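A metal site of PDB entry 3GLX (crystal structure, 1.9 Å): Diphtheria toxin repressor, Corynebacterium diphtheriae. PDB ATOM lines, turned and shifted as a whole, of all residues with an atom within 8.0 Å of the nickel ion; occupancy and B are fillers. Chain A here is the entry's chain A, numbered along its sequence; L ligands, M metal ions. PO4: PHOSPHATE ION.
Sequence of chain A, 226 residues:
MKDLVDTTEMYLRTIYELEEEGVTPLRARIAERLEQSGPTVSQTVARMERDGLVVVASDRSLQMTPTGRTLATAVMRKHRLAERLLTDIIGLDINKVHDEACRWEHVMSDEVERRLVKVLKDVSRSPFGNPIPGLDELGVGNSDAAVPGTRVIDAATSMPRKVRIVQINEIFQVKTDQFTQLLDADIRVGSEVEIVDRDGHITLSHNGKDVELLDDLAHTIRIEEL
The nickel ion is bound by OE2 of Glu 83 (2.0 Å), O2 of the ligand (2.0 Å), ND1 of His 98 (2.0 Å) and NE2 of His 79 (2.2 Å).
Three residues have an atom within 4 Å of the nickel ion: His 79, Glu 83 and His 98. Along chain A the residues within 4 Å of the nickel ion span positions 79 to 98. The nearest printed residue that does not touch the nickel ion is Phe 128 (4.2 Å).
NE2 of His 98 lies within hydrogen-bond range of SG of Cys 102. ND1 of His 79 sits at hydrogen-bond distance from NH2 of Arg 13. A ring nitrogen (ND1) of His 79 sits at hydrogen-bond distance from the backbone carbonyl oxygen of Ala 101, 3.3 Å away. OE1 of Glu 105 sits at hydrogen-bond distance from ND1 of His 79.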
ATOM      1  N   ARG A  13      -7.681   9.637   6.890  1.00  0.00           N
ATOM      2  CA  ARG A  13      -6.231   9.702   6.714  1.00  0.00           C
ATOM      3  C   ARG A  13      -5.718   8.839   5.551  1.00  0.00           C
ATOM      4  O   ARG A  13      -4.691   9.152   4.972  1.00  0.00           O
ATOM      5  CB  ARG A  13      -5.420   9.429   8.018  1.00  0.00           C
ATOM      6  CG  ARG A  13      -5.616   8.091   8.594  1.00  0.00           C
ATOM      7  CD  ARG A  13      -4.500   7.110   8.262  1.00  0.00           C
ATOM      8  NE  ARG A  13      -3.260   7.506   8.958  1.00  0.00           N
ATOM      9  CZ  ARG A  13      -2.092   7.616   8.363  1.00  0.00           C
ATOM     10  NH1 ARG A  13      -1.962   7.371   7.053  1.00  0.00           N
ATOM     11  NH2 ARG A  13      -1.043   7.953   9.073  1.00  0.00           N
ATOM     12  N   GLU A  17      -3.542  10.131   2.384  1.00  0.00           N
ATOM     13  CA  GLU A  17      -2.227   9.553   2.083  1.00  0.00           C
ATOM     14  C   GLU A  17      -2.190   9.105   0.610  1.00  0.00           C
ATOM     15  O   GLU A  17      -1.215   9.346  -0.141  1.00  0.00           O
ATOM     16  CB  GLU A  17      -2.050   8.375   3.031  1.00  0.00           C
ATOM     17  CG  GLU A  17      -0.666   7.878   3.209  1.00  0.00           C
ATOM     18  CD  GLU A  17      -0.695   6.623   4.061  1.00  0.00           C
ATOM     19  OE1 GLU A  17      -1.651   5.818   3.942  1.00  0.00           O
ATOM     20  OE2 GLU A  17       0.241   6.448   4.825  1.00  0.00           O
ATOM     21  N   MET A  76      -3.401  13.556  10.086  1.00  0.00           N
ATOM     22  CA  MET A  76      -2.024  13.470   9.523  1.00  0.00           C
ATOM     23  C   MET A  76      -0.988  14.282  10.288  1.00  0.00           C
ATOM     24  O   MET A  76       0.155  13.825  10.459  1.00  0.00           O
ATOM     25  CB  MET A  76      -2.019  13.886   8.070  1.00  0.00           C
ATOM     26  CG  MET A  76      -0.703  13.494   7.313  1.00  0.00           C
ATOM     27  SD  MET A  76      -0.371  11.697   7.274  1.00  0.00           S
ATOM     28  CE  MET A  76      -2.191  11.106   7.236  1.00  0.00           C
ATOM     29  N   HIS A  79      -0.218  12.338  13.394  1.00  0.00           N
ATOM     30  CA  HIS A  79       0.600  11.193  13.006  1.00  0.00           C
ATOM     31  C   HIS A  79       2.079  11.635  12.835  1.00  0.00           C
ATOM     32  O   HIS A  79       3.024  11.033  13.423  1.00  0.00           O
ATOM     33  CB  HIS A  79       0.072  10.672  11.642  1.00  0.00           C
ATOM     34  CG  HIS A  79       0.835   9.521  11.135  1.00  0.00           C
ATOM     35  ND1 HIS A  79       0.642   8.255  11.649  1.00  0.00           N
ATOM     36  CD2 HIS A  79       1.819   9.414  10.190  1.00  0.00           C
ATOM     37  CE1 HIS A  79       1.451   7.403  11.029  1.00  0.00           C
ATOM     38  NE2 HIS A  79       2.181   8.085  10.164  1.00  0.00           N
ATOM     39  N   ARG A  80       2.273  12.711  12.092  1.00  0.00           N
ATOM     40  CA  ARG A  80       3.648  13.170  11.796  1.00  0.00           C
ATOM     41  C   ARG A  80       4.416  13.802  12.954  1.00  0.00           C
ATOM     42  O   ARG A  80       5.651  13.623  13.111  1.00  0.00           O
ATOM     43  CB  ARG A  80       3.637  14.032  10.493  1.00  0.00           C
ATOM     44  CG  ARG A  80       3.239  13.141   9.343  1.00  0.00           C
ATOM     45  CD  ARG A  80       3.242  13.818   7.962  1.00  0.00           C
ATOM     46  NE  ARG A  80       2.927  12.818   6.960  1.00  0.00           N
ATOM     47  CZ  ARG A  80       2.513  13.036   5.719  1.00  0.00           C
ATOM     48  NH1 ARG A  80       2.294  14.259   5.255  1.00  0.00           N
ATOM     49  NH2 ARG A  80       2.277  11.993   4.958  1.00  0.00           N
ATOM     50  N   GLU A  83       5.516  10.866  14.963  1.00  0.00           N
ATOM     51  CA  GLU A  83       6.743  10.297  14.398  1.00  0.00           C
ATOM     52  C   GLU A  83       7.947  11.105  14.782  1.00  0.00           C
ATOM     53  O   GLU A  83       8.983  10.531  15.120  1.00  0.00           O
ATOM     54  CB  GLU A  83       6.613  10.190  12.868  1.00  0.00           C
ATOM     55  CG  GLU A  83       5.647   9.129  12.531  1.00  0.00           C
ATOM     56  CD  GLU A  83       5.497   8.921  10.989  1.00  0.00           C
ATOM     57  OE1 GLU A  83       5.550   9.928  10.259  1.00  0.00           O
ATOM     58  OE2 GLU A  83       5.247   7.801  10.539  1.00  0.00           O
ATOM     59  N   VAL A  97       8.545   3.090  13.956  1.00  0.00           N
ATOM     60  CA  VAL A  97       8.031   4.477  14.255  1.00  0.00           C
ATOM     61  C   VAL A  97       6.683   4.698  13.529  1.00  0.00           C
ATOM     62  O   VAL A  97       5.693   5.110  14.171  1.00  0.00           O
ATOM     63  CB  VAL A  97       9.089   5.533  13.881  1.00  0.00           C
ATOM     64  CG1 VAL A  97       8.440   6.937  13.624  1.00  0.00           C
ATOM     65  CG2 VAL A  97      10.118   5.548  15.045  1.00  0.00           C
ATOM     66  N   HIS A  98       6.602   4.351  12.230  1.00  0.00           N
ATOM     67  CA  HIS A  98       5.344   4.565  11.495  1.00  0.00           C
ATOM     68  C   HIS A  98       4.154   3.785  12.118  1.00  0.00           C
ATOM     69  O   HIS A  98       3.090   4.372  12.402  1.00  0.00           O
ATOM     70  CB  HIS A  98       5.484   4.275   9.961  1.00  0.00           C
ATOM     71  CG  HIS A  98       4.165   4.283   9.242  1.00  0.00           C
ATOM     72  ND1 HIS A  98       3.489   5.445   8.917  1.00  0.00           N
ATOM     73  CD2 HIS A  98       3.374   3.265   8.811  1.00  0.00           C
ATOM     74  CE1 HIS A  98       2.356   5.142   8.298  1.00  0.00           C
ATOM     75  NE2 HIS A  98       2.269   3.832   8.226  1.00  0.00           N
ATOM     76  N   ASP A  99       4.371   2.506  12.427  1.00  0.00           N
ATOM     77  CA  ASP A  99       3.295   1.671  12.964  1.00  0.00           C
ATOM     78  C   ASP A  99       2.871   2.146  14.365  1.00  0.00           C
ATOM     79  O   ASP A  99       1.687   2.123  14.651  1.00  0.00           O
ATOM     80  CB  ASP A  99       3.731   0.195  13.074  1.00  0.00           C
ATOM     81  CG  ASP A  99       3.863  -0.469  11.695  1.00  0.00           C
ATOM     82  OD1 ASP A  99       3.267   0.050  10.719  1.00  0.00           O
ATOM     83  OD2 ASP A  99       4.649  -1.455  11.598  1.00  0.00           O
ATOM     84  N   GLU A 100       3.825   2.616  15.177  1.00  0.00           N
ATOM     85  CA  GLU A 100       3.495   3.242  16.504  1.00  0.00           C
ATOM     86  C   GLU A 100       2.633   4.508  16.308  1.00  0.00           C
ATOM     87  O   GLU A 100       1.593   4.683  16.936  1.00  0.00           O
ATOM     88  CB  GLU A 100       4.781   3.582  17.279  1.00  0.00           C
ATOM     89  CG  GLU A 100       4.674   3.903  18.750  1.00  0.00           C
ATOM     90  CD  GLU A 100       4.551   2.672  19.689  1.00  0.00           C
ATOM     91  OE1 GLU A 100       5.253   1.656  19.452  1.00  0.00           O
ATOM     92  OE2 GLU A 100       3.853   2.781  20.741  1.00  0.00           O
ATOM     93  N   ALA A 101       3.044   5.378  15.395  1.00  0.00           N
ATOM     94  CA  ALA A 101       2.376   6.652  15.116  1.00  0.00           C
ATOM     95  C   ALA A 101       1.001   6.416  14.538  1.00  0.00           C
ATOM     96  O   ALA A 101       0.080   7.221  14.772  1.00  0.00           O
ATOM     97  CB  ALA A 101       3.243   7.493  14.119  1.00  0.00           C
ATOM     98  N   CYS A 102       0.814   5.323  13.806  1.00  0.00           N
ATOM     99  CA  CYS A 102      -0.554   5.015  13.290  1.00  0.00           C
ATOM    100  C   CYS A 102      -1.576   4.832  14.424  1.00  0.00           C
ATOM    101  O   CYS A 102      -2.768   5.016  14.218  1.00  0.00           O
ATOM    102  CB  CYS A 102      -0.556   3.743  12.468  1.00  0.00           C
ATOM    103  SG  CYS A 102       0.099   4.074  10.818  1.00  0.00           S
ATOM    104  N   GLU A 105      -1.801   8.629  16.506  1.00  0.00           N
ATOM    105  CA  GLU A 105      -2.503   9.754  15.864  1.00  0.00           C
ATOM    106  C   GLU A 105      -3.945   9.873  16.319  1.00  0.00           C
ATOM    107  O   GLU A 105      -4.540  10.972  16.199  1.00  0.00           O
ATOM    108  CB  GLU A 105      -2.423   9.600  14.328  1.00  0.00           C
ATOM    109  CG  GLU A 105      -3.213   8.401  13.872  1.00  0.00           C
ATOM    110  CD  GLU A 105      -2.985   8.035  12.381  1.00  0.00           C
ATOM    111  OE1 GLU A 105      -1.890   8.203  11.864  1.00  0.00           O
ATOM    112  OE2 GLU A 105      -3.918   7.558  11.757  1.00  0.00           O
ATOM    113  N   SER A 126       7.948  14.940   8.373  1.00  0.00           N
ATOM    114  CA  SER A 126       8.074  13.690   9.117  1.00  0.00           C
ATOM    115  C   SER A 126       9.485  13.104   8.912  1.00  0.00           C
ATOM    116  O   SER A 126      10.256  13.570   8.034  1.00  0.00           O
ATOM    117  CB  SER A 126       7.034  12.646   8.656  1.00  0.00           C
ATOM    118  OG  SER A 126       7.421  12.038   7.411  1.00  0.00           O
ATOM    119  N   PRO A 127       9.820  12.095   9.700  1.00  0.00           N
ATOM    120  CA  PRO A 127      11.133  11.419   9.441  1.00  0.00           C
ATOM    121  C   PRO A 127      11.195  10.702   8.063  1.00  0.00           C
ATOM    122  O   PRO A 127      12.286  10.273   7.641  1.00  0.00           O
ATOM    123  CB  PRO A 127      11.213  10.330  10.539  1.00  0.00           C
ATOM    124  CG  PRO A 127      10.212  10.744  11.642  1.00  0.00           C
ATOM    125  CD  PRO A 127       9.114  11.568  10.908  1.00  0.00           C
ATOM    126  N   PHE A 128      10.043  10.537   7.433  1.00  0.00           N
ATOM    127  CA  PHE A 128       9.938   9.790   6.206  1.00  0.00           C
ATOM    128  C   PHE A 128       9.782  10.698   5.016  1.00  0.00           C
ATOM    129  O   PHE A 128       9.391  10.213   3.942  1.00  0.00           O
ATOM    130  CB  PHE A 128       8.790   8.760   6.363  1.00  0.00           C
ATOM    131  CG  PHE A 128       9.006   7.858   7.569  1.00  0.00           C
ATOM    132  CD1 PHE A 128      10.143   7.043   7.646  1.00  0.00           C
ATOM    133  CD2 PHE A 128       8.106   7.844   8.636  1.00  0.00           C
ATOM    134  CE1 PHE A 128      10.393   6.222   8.763  1.00  0.00           C
ATOM    135  CE2 PHE A 128       8.357   7.049   9.740  1.00  0.00           C
ATOM    136  CZ  PHE A 128       9.494   6.224   9.814  1.00  0.00           C
ATOM    137  N   ASN A 130       7.857  13.612   4.432  1.00  0.00           N
ATOM    138  CA  ASN A 130       6.626  14.261   3.983  1.00  0.00           C
ATOM    139  C   ASN A 130       6.295  15.461   4.883  1.00  0.00           C
ATOM    140  O   ASN A 130       6.532  15.420   6.056  1.00  0.00           O
ATOM    141  CB  ASN A 130       5.474  13.224   3.992  1.00  0.00           C
ATOM    142  CG  ASN A 130       5.692  12.129   2.952  1.00  0.00           C
ATOM    143  OD1 ASN A 130       5.608  10.923   3.249  1.00  0.00           O
ATOM    144  ND2 ASN A 130       6.047  12.540   1.733  1.00  0.00           N
HETATM  145  P   PO4 L   1       4.605   9.434   6.827  1.00  0.00           P
HETATM  146  O1  PO4 L   1       5.051   9.423   5.385  1.00  0.00           O
HETATM  147  O2  PO4 L   1       4.679   8.042   7.388  1.00  0.00           O
HETATM  148  O3  PO4 L   1       3.191   9.863   6.867  1.00  0.00           O
HETATM  149  O4  PO4 L   1       5.542  10.315   7.568  1.00  0.00           O
HETATM  150 NI    NI M   1       3.971   7.396   9.104  1.00  0.00          NI
